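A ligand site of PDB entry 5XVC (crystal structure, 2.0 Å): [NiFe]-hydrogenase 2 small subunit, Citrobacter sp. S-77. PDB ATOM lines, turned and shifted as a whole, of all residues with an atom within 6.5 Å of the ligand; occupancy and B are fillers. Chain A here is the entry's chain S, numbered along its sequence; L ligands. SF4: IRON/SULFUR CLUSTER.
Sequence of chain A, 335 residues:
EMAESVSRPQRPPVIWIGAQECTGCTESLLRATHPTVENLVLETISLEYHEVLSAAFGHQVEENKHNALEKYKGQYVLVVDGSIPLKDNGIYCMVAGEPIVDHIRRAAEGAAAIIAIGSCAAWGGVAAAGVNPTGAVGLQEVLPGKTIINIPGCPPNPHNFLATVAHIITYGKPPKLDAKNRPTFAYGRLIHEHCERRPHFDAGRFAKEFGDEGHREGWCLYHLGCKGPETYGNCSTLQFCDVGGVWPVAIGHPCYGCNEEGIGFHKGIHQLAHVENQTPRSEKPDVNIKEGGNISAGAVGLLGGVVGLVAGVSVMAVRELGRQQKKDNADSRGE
A ring nitrogen (ND1) of His 192 is bound to an iron atom (FE3) of the ligand, 2.3 Å away. The side-chain sulfur (SG) of Cys 195 binds an iron atom (FE2) of the ligand. FE1 of the ligand is bound by SG of Cys 220 (2.3 Å). S3 of the ligand sits close to N of Leu 221 (3.7 Å). The side-chain sulfur (SG) of Cys 226 is bound to an iron atom (FE4) of the ligand (2.3 Å). The backbone NH (N) of Arg 198 sits close to a sulfur (S4) of the ligand, at 3.6 Å.
SG of Cys 226 sits close to N of Gly 228 (3.3 Å). The backbone carbonyl oxygen (O) of Gly 228 sits at hydrogen-bond distance from the backbone NH (N) of His 192 (3.2 Å). SG of Cys 226 lies close to N of Cys 255, 3.5 Å away. NH2 of Arg 197 is in hydrogen-bond range of O of Val 249 (3.1 Å). N of Arg 197 sits close to SG of Cys 195, 3.5 Å away. NH1 of Arg 198 sits at hydrogen-bond distance from NE2 of His 192 (3.1 Å). The side-chain sulfur of Cys 220 lies close to the backbone NH of Tyr 222 (3.2 Å). The guanidinium group (NH1) of Arg 197 lies within hydrogen-bond range of the backbone carbonyl oxygen (O) of Trp 219 (2.9 Å).
Residues that only touch the ligand: Arg 197, Tyr 222, Gly 228 and Pro 229. Hydrophobic or aromatic side chains within 4 Å of the ligand: His 192, Tyr 222 and Pro 229. Within 4 Å of the ligand: His 192, Cys 195, Arg 197, Arg 198, Cys 220, Leu 221, Tyr 222, Cys 226, Gly 228 and Pro 229.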
ATOM      1  N   ILE A 191      -6.294 -25.686  13.818  1.00  0.00           N
ATOM      2  CA  ILE A 191      -7.375 -25.972  12.897  1.00  0.00           C
ATOM      3  C   ILE A 191      -7.136 -25.185  11.600  1.00  0.00           C
ATOM      4  O   ILE A 191      -7.303 -25.712  10.510  1.00  0.00           O
ATOM      5  CB  ILE A 191      -8.771 -25.657  13.517  1.00  0.00           C
ATOM      6  CG1 ILE A 191      -9.164 -26.735  14.545  1.00  0.00           C
ATOM      7  CG2 ILE A 191      -9.837 -25.539  12.440  1.00  0.00           C
ATOM      8  CD1 ILE A 191     -10.192 -26.245  15.594  1.00  0.00           C
ATOM      9  N   HIS A 192      -6.707 -23.936  11.749  1.00  0.00           N
ATOM     10  CA  HIS A 192      -6.414 -23.027  10.627  1.00  0.00           C
ATOM     11  C   HIS A 192      -5.266 -23.501   9.712  1.00  0.00           C
ATOM     12  O   HIS A 192      -5.184 -23.080   8.564  1.00  0.00           O
ATOM     13  CB  HIS A 192      -6.079 -21.644  11.205  1.00  0.00           C
ATOM     14  CG  HIS A 192      -5.647 -20.607  10.197  1.00  0.00           C
ATOM     15  ND1 HIS A 192      -6.542 -19.931   9.394  1.00  0.00           N
ATOM     16  CD2 HIS A 192      -4.430 -20.104   9.896  1.00  0.00           C
ATOM     17  CE1 HIS A 192      -5.886 -19.074   8.632  1.00  0.00           C
ATOM     18  NE2 HIS A 192      -4.603 -19.155   8.919  1.00  0.00           N
ATOM     19  N   GLU A 193      -4.380 -24.331  10.243  1.00  0.00           N
ATOM     20  CA  GLU A 193      -3.270 -24.870   9.448  1.00  0.00           C
ATOM     21  C   GLU A 193      -3.647 -26.176   8.720  1.00  0.00           C
ATOM     22  O   GLU A 193      -2.814 -26.827   8.078  1.00  0.00           O
ATOM     23  CB  GLU A 193      -2.005 -25.066  10.309  1.00  0.00           C
ATOM     24  CG  GLU A 193      -1.313 -23.740  10.707  1.00  0.00           C
ATOM     25  CD  GLU A 193      -0.951 -22.887   9.487  1.00  0.00           C
ATOM     26  OE1 GLU A 193      -0.111 -23.324   8.673  1.00  0.00           O
ATOM     27  OE2 GLU A 193      -1.532 -21.789   9.334  1.00  0.00           O
ATOM     28  N   CYS A 195      -7.277 -26.218   7.331  1.00  0.00           N
ATOM     29  CA  CYS A 195      -8.671 -25.879   7.040  1.00  0.00           C
ATOM     30  C   CYS A 195      -8.956 -25.621   5.576  1.00  0.00           C
ATOM     31  O   CYS A 195      -8.239 -24.868   4.901  1.00  0.00           O
ATOM     32  CB  CYS A 195      -9.116 -24.654   7.841  1.00  0.00           C
ATOM     33  SG  CYS A 195     -10.851 -24.289   7.456  1.00  0.00           S
ATOM     34  N   GLU A 196     -10.062 -26.207   5.105  1.00  0.00           N
ATOM     35  CA  GLU A 196     -10.411 -26.249   3.691  1.00  0.00           C
ATOM     36  C   GLU A 196     -10.786 -24.883   3.121  1.00  0.00           C
ATOM     37  O   GLU A 196     -10.817 -24.718   1.904  1.00  0.00           O
ATOM     38  CB  GLU A 196     -11.524 -27.285   3.444  1.00  0.00           C
ATOM     39  CG  GLU A 196     -12.918 -26.902   4.022  1.00  0.00           C
ATOM     40  CD  GLU A 196     -13.214 -27.466   5.408  1.00  0.00           C
ATOM     41  OE1 GLU A 196     -12.251 -27.758   6.147  1.00  0.00           O
ATOM     42  OE2 GLU A 196     -14.418 -27.603   5.747  1.00  0.00           O
ATOM     43  N   ARG A 197     -11.038 -23.896   3.990  1.00  0.00           N
ATOM     44  CA  ARG A 197     -11.341 -22.539   3.532  1.00  0.00           C
ATOM     45  C   ARG A 197     -10.121 -21.618   3.516  1.00  0.00           C
ATOM     46  O   ARG A 197     -10.203 -20.474   3.091  1.00  0.00           O
ATOM     47  CB  ARG A 197     -12.514 -21.913   4.331  1.00  0.00           C
ATOM     48  CG  ARG A 197     -13.741 -22.840   4.348  1.00  0.00           C
ATOM     49  CD  ARG A 197     -14.954 -22.228   5.016  1.00  0.00           C
ATOM     50  NE  ARG A 197     -16.115 -23.114   4.840  1.00  0.00           N
ATOM     51  CZ  ARG A 197     -17.387 -22.713   4.861  1.00  0.00           C
ATOM     52  NH1 ARG A 197     -17.698 -21.431   5.042  1.00  0.00           N
ATOM     53  NH2 ARG A 197     -18.352 -23.607   4.682  1.00  0.00           N
ATOM     54  N   ARG A 198      -8.967 -22.125   3.953  1.00  0.00           N
ATOM     55  CA  ARG A 198      -7.708 -21.399   3.792  1.00  0.00           C
ATOM     56  C   ARG A 198      -7.507 -20.698   2.420  1.00  0.00           C
ATOM     57  O   ARG A 198      -7.014 -19.555   2.379  1.00  0.00           O
ATOM     58  CB  ARG A 198      -6.506 -22.299   4.138  1.00  0.00           C
ATOM     59  CG  ARG A 198      -5.152 -21.571   4.153  1.00  0.00           C
ATOM     60  CD  ARG A 198      -5.089 -20.465   5.225  1.00  0.00           C
ATOM     61  NE  ARG A 198      -3.756 -19.875   5.269  1.00  0.00           N
ATOM     62  CZ  ARG A 198      -2.815 -20.204   6.154  1.00  0.00           C
ATOM     63  NH1 ARG A 198      -3.066 -21.119   7.094  1.00  0.00           N
ATOM     64  NH2 ARG A 198      -1.615 -19.625   6.102  1.00  0.00           N
ATOM     65  N   PRO A 199      -7.893 -21.343   1.304  1.00  0.00           N
ATOM     66  CA  PRO A 199      -7.705 -20.617   0.038  1.00  0.00           C
ATOM     67  C   PRO A 199      -8.534 -19.340  -0.046  1.00  0.00           C
ATOM     68  O   PRO A 199      -8.165 -18.364  -0.728  1.00  0.00           O
ATOM     69  CB  PRO A 199      -8.204 -21.595  -1.006  1.00  0.00           C
ATOM     70  CG  PRO A 199      -7.996 -22.935  -0.390  1.00  0.00           C
ATOM     71  CD  PRO A 199      -8.322 -22.738   1.062  1.00  0.00           C
ATOM     72  N   PHE A 201      -9.450 -17.525   2.696  1.00  0.00           N
ATOM     73  CA  PHE A 201      -8.696 -16.636   3.603  1.00  0.00           C
ATOM     74  C   PHE A 201      -7.535 -15.949   2.861  1.00  0.00           C
ATOM     75  O   PHE A 201      -7.364 -14.734   2.961  1.00  0.00           O
ATOM     76  CB  PHE A 201      -8.157 -17.446   4.786  1.00  0.00           C
ATOM     77  CG  PHE A 201      -7.283 -16.657   5.735  1.00  0.00           C
ATOM     78  CD1 PHE A 201      -7.848 -16.004   6.820  1.00  0.00           C
ATOM     79  CD2 PHE A 201      -5.915 -16.594   5.556  1.00  0.00           C
ATOM     80  CE1 PHE A 201      -7.043 -15.295   7.707  1.00  0.00           C
ATOM     81  CE2 PHE A 201      -5.120 -15.890   6.422  1.00  0.00           C
ATOM     82  CZ  PHE A 201      -5.686 -15.238   7.507  1.00  0.00           C
ATOM     83  N   PHE A 206     -14.190 -13.425   2.203  1.00  0.00           N
ATOM     84  CA  PHE A 206     -14.704 -13.599   3.555  1.00  0.00           C
ATOM     85  C   PHE A 206     -16.201 -13.455   3.603  1.00  0.00           C
ATOM     86  O   PHE A 206     -16.760 -12.668   2.860  1.00  0.00           O
ATOM     87  CB  PHE A 206     -14.102 -12.553   4.480  1.00  0.00           C
ATOM     88  CG  PHE A 206     -12.632 -12.685   4.690  1.00  0.00           C
ATOM     89  CD1 PHE A 206     -12.124 -13.784   5.372  1.00  0.00           C
ATOM     90  CD2 PHE A 206     -11.755 -11.732   4.206  1.00  0.00           C
ATOM     91  CE1 PHE A 206     -10.768 -13.925   5.573  1.00  0.00           C
ATOM     92  CE2 PHE A 206     -10.378 -11.866   4.409  1.00  0.00           C
ATOM     93  CZ  PHE A 206      -9.893 -12.952   5.104  1.00  0.00           C
ATOM     94  N   TRP A 219     -17.300 -19.194   1.749  1.00  0.00           N
ATOM     95  CA  TRP A 219     -16.021 -18.516   1.926  1.00  0.00           C
ATOM     96  C   TRP A 219     -15.565 -18.574   3.380  1.00  0.00           C
ATOM     97  O   TRP A 219     -16.279 -19.056   4.248  1.00  0.00           O
ATOM     98  CB  TRP A 219     -16.111 -17.067   1.457  1.00  0.00           C
ATOM     99  CG  TRP A 219     -16.234 -16.903  -0.032  1.00  0.00           C
ATOM    100  CD1 TRP A 219     -16.175 -17.892  -0.979  1.00  0.00           C
ATOM    101  CD2 TRP A 219     -16.440 -15.679  -0.739  1.00  0.00           C
ATOM    102  NE1 TRP A 219     -16.344 -17.351  -2.232  1.00  0.00           N
ATOM    103  CE2 TRP A 219     -16.513 -15.994  -2.112  1.00  0.00           C
ATOM    104  CE3 TRP A 219     -16.559 -14.334  -0.350  1.00  0.00           C
ATOM    105  CZ2 TRP A 219     -16.701 -15.028  -3.086  1.00  0.00           C
ATOM    106  CZ3 TRP A 219     -16.763 -13.379  -1.314  1.00  0.00           C
ATOM    107  CH2 TRP A 219     -16.832 -13.728  -2.675  1.00  0.00           C
ATOM    108  N   CYS A 220     -14.383 -18.050   3.640  1.00  0.00           N
ATOM    109  CA  CYS A 220     -13.763 -18.112   4.945  1.00  0.00           C
ATOM    110  C   CYS A 220     -14.550 -17.306   5.994  1.00  0.00           C
ATOM    111  O   CYS A 220     -15.163 -16.280   5.666  1.00  0.00           O
ATOM    112  CB  CYS A 220     -12.323 -17.612   4.835  1.00  0.00           C
ATOM    113  SG  CYS A 220     -11.576 -17.294   6.408  1.00  0.00           S
ATOM    114  N   LEU A 221     -14.549 -17.795   7.232  1.00  0.00           N
ATOM    115  CA  LEU A 221     -15.344 -17.218   8.308  1.00  0.00           C
ATOM    116  C   LEU A 221     -14.505 -16.386   9.291  1.00  0.00           C
ATOM    117  O   LEU A 221     -15.008 -15.984  10.370  1.00  0.00           O
ATOM    118  CB  LEU A 221     -16.077 -18.319   9.078  1.00  0.00           C
ATOM    119  CG  LEU A 221     -16.912 -19.304   8.250  1.00  0.00           C
ATOM    120  CD1 LEU A 221     -17.723 -20.246   9.136  1.00  0.00           C
ATOM    121  CD2 LEU A 221     -17.827 -18.580   7.257  1.00  0.00           C
ATOM    122  N   TYR A 222     -13.244 -16.118   8.932  1.00  0.00           N
ATOM    123  CA  TYR A 222     -12.341 -15.338   9.805  1.00  0.00           C
ATOM    124  C   TYR A 222     -13.004 -14.091  10.357  1.00  0.00           C
ATOM    125  O   TYR A 222     -12.951 -13.815  11.568  1.00  0.00           O
ATOM    126  CB  TYR A 222     -11.019 -14.935   9.097  1.00  0.00           C
ATOM    127  CG  TYR A 222     -10.125 -14.166  10.056  1.00  0.00           C
ATOM    128  CD1 TYR A 222      -9.394 -14.822  11.036  1.00  0.00           C
ATOM    129  CD2 TYR A 222     -10.053 -12.779  10.010  1.00  0.00           C
ATOM    130  CE1 TYR A 222      -8.601 -14.110  11.952  1.00  0.00           C
ATOM    131  CE2 TYR A 222      -9.256 -12.074  10.908  1.00  0.00           C
ATOM    132  CZ  TYR A 222      -8.530 -12.756  11.873  1.00  0.00           C
ATOM    133  OH  TYR A 222      -7.758 -12.051  12.787  1.00  0.00           O
ATOM    134  N   HIS A 223     -13.637 -13.340   9.472  1.00  0.00           N
ATOM    135  CA  HIS A 223     -14.187 -12.054   9.884  1.00  0.00           C
ATOM    136  C   HIS A 223     -15.535 -12.127  10.602  1.00  0.00           C
ATOM    137  O   HIS A 223     -16.074 -11.119  11.049  1.00  0.00           O
ATOM    138  CB  HIS A 223     -14.214 -11.077   8.713  1.00  0.00           C
ATOM    139  CG  HIS A 223     -12.872 -10.469   8.445  1.00  0.00           C
ATOM    140  ND1 HIS A 223     -12.318  -9.516   9.272  1.00  0.00           N
ATOM    141  CD2 HIS A 223     -11.960 -10.702   7.464  1.00  0.00           C
ATOM    142  CE1 HIS A 223     -11.122  -9.185   8.808  1.00  0.00           C
ATOM    143  NE2 HIS A 223     -10.889  -9.889   7.720  1.00  0.00           N
ATOM    144  N   CYS A 226     -14.022 -16.452  13.455  1.00  0.00           N
ATOM    145  CA  CYS A 226     -13.454 -17.802  13.503  1.00  0.00           C
ATOM    146  C   CYS A 226     -12.162 -17.870  14.309  1.00  0.00           C
ATOM    147  O   CYS A 226     -11.208 -17.109  14.090  1.00  0.00           O
ATOM    148  CB  CYS A 226     -13.224 -18.382  12.110  1.00  0.00           C
ATOM    149  SG  CYS A 226     -12.685 -20.078  12.281  1.00  0.00           S
ATOM    150  N   LYS A 227     -12.118 -18.813  15.249  1.00  0.00           N
ATOM    151  CA  LYS A 227     -10.967 -18.959  16.105  1.00  0.00           C
ATOM    152  C   LYS A 227     -10.021 -20.048  15.632  1.00  0.00           C
ATOM    153  O   LYS A 227      -9.054 -20.382  16.310  1.00  0.00           O
ATOM    154  CB  LYS A 227     -11.399 -19.214  17.551  1.00  0.00           C
ATOM    155  CG  LYS A 227     -12.313 -18.120  18.124  1.00  0.00           C
ATOM    156  CD  LYS A 227     -11.695 -16.740  17.938  1.00  0.00           C
ATOM    157  CE  LYS A 227     -12.411 -15.714  18.825  1.00  0.00           C
ATOM    158  NZ  LYS A 227     -13.813 -15.502  18.380  1.00  0.00           N
ATOM    159  N   GLY A 228     -10.307 -20.601  14.452  1.00  0.00           N
ATOM    160  CA  GLY A 228      -9.407 -21.536  13.816  1.00  0.00           C
ATOM    161  C   GLY A 228      -7.925 -21.166  13.925  1.00  0.00           C
ATOM    162  O   GLY A 228      -7.125 -22.024  14.267  1.00  0.00           O
ATOM    163  N   PRO A 229      -7.563 -19.883  13.678  1.00  0.00           N
ATOM    164  CA  PRO A 229      -6.139 -19.493  13.791  1.00  0.00           C
ATOM    165  C   PRO A 229      -5.487 -19.721  15.143  1.00  0.00           C
ATOM    166  O   PRO A 229      -4.257 -19.768  15.185  1.00  0.00           O
ATOM    167  CB  PRO A 229      -6.177 -17.997  13.466  1.00  0.00           C
ATOM    168  CG  PRO A 229      -7.283 -17.886  12.480  1.00  0.00           C
ATOM    169  CD  PRO A 229      -8.347 -18.837  13.003  1.00  0.00           C
ATOM    170  N   TRP A 247     -18.584 -30.171  10.492  1.00  0.00           N
ATOM    171  CA  TRP A 247     -17.987 -29.461  11.606  1.00  0.00           C
ATOM    172  C   TRP A 247     -18.557 -28.059  11.606  1.00  0.00           C
ATOM    173  O   TRP A 247     -19.262 -27.685  10.655  1.00  0.00           O
ATOM    174  CB  TRP A 247     -16.456 -29.536  11.575  1.00  0.00           C
ATOM    175  CG  TRP A 247     -15.724 -28.814  10.477  1.00  0.00           C
ATOM    176  CD1 TRP A 247     -15.766 -29.071   9.134  1.00  0.00           C
ATOM    177  CD2 TRP A 247     -14.763 -27.750  10.655  1.00  0.00           C
ATOM    178  NE1 TRP A 247     -14.918 -28.208   8.460  1.00  0.00           N
ATOM    179  CE2 TRP A 247     -14.281 -27.399   9.369  1.00  0.00           C
ATOM    180  CE3 TRP A 247     -14.283 -27.059  11.774  1.00  0.00           C
ATOM    181  CZ2 TRP A 247     -13.316 -26.392   9.183  1.00  0.00           C
ATOM    182  CZ3 TRP A 247     -13.332 -26.053  11.585  1.00  0.00           C
ATOM    183  CH2 TRP A 247     -12.870 -25.724  10.292  1.00  0.00           C
ATOM    184  N   VAL A 249     -17.497 -24.916  11.016  1.00  0.00           N
ATOM    185  CA  VAL A 249     -17.367 -23.992   9.880  1.00  0.00           C
ATOM    186  C   VAL A 249     -17.909 -24.557   8.572  1.00  0.00           C
ATOM    187  O   VAL A 249     -18.438 -23.796   7.747  1.00  0.00           O
ATOM    188  CB  VAL A 249     -15.992 -23.259   9.718  1.00  0.00           C
ATOM    189  CG1 VAL A 249     -15.161 -23.243  11.017  1.00  0.00           C
ATOM    190  CG2 VAL A 249     -15.260 -23.735   8.524  1.00  0.00           C
ATOM    191  N   PRO A 254     -18.402 -19.781  12.567  1.00  0.00           N
ATOM    192  CA  PRO A 254     -16.996 -19.762  12.973  1.00  0.00           C
ATOM    193  C   PRO A 254     -16.675 -20.757  14.077  1.00  0.00           C
ATOM    194  O   PRO A 254     -17.532 -21.036  14.919  1.00  0.00           O
ATOM    195  CB  PRO A 254     -16.807 -18.311  13.493  1.00  0.00           C
ATOM    196  CG  PRO A 254     -18.212 -17.755  13.727  1.00  0.00           C
ATOM    197  CD  PRO A 254     -19.041 -18.457  12.663  1.00  0.00           C
ATOM    198  N   CYS A 255     -15.469 -21.324  14.054  1.00  0.00           N
ATOM    199  CA  CYS A 255     -14.914 -21.942  15.243  1.00  0.00           C
ATOM    200  C   CYS A 255     -14.947 -20.915  16.396  1.00  0.00           C
ATOM    201  O   CYS A 255     -14.672 -19.726  16.184  1.00  0.00           O
ATOM    202  CB  CYS A 255     -13.495 -22.426  14.978  1.00  0.00           C
ATOM    203  SG  CYS A 255     -12.579 -23.000  16.424  1.00  0.00           S
HETATM  204 FE1  SF4 L   1     -10.944 -19.146   7.667  1.00  0.00          FE
HETATM  205 FE2  SF4 L   1     -10.798 -21.983   8.110  1.00  0.00          FE
HETATM  206 FE3  SF4 L   1      -8.807 -20.216   9.208  1.00  0.00          FE
HETATM  207 FE4  SF4 L   1     -11.446 -20.312  10.309  1.00  0.00          FE
HETATM  208  S1  SF4 L   1      -9.951 -21.883  10.088  1.00  0.00           S
HETATM  209  S2  SF4 L   1     -10.207 -18.620   9.684  1.00  0.00           S
HETATM  210  S3  SF4 L   1     -12.452 -20.587   8.398  1.00  0.00           S
HETATM  211  S4  SF4 L   1      -9.417 -20.590   7.136  1.00  0.00           S
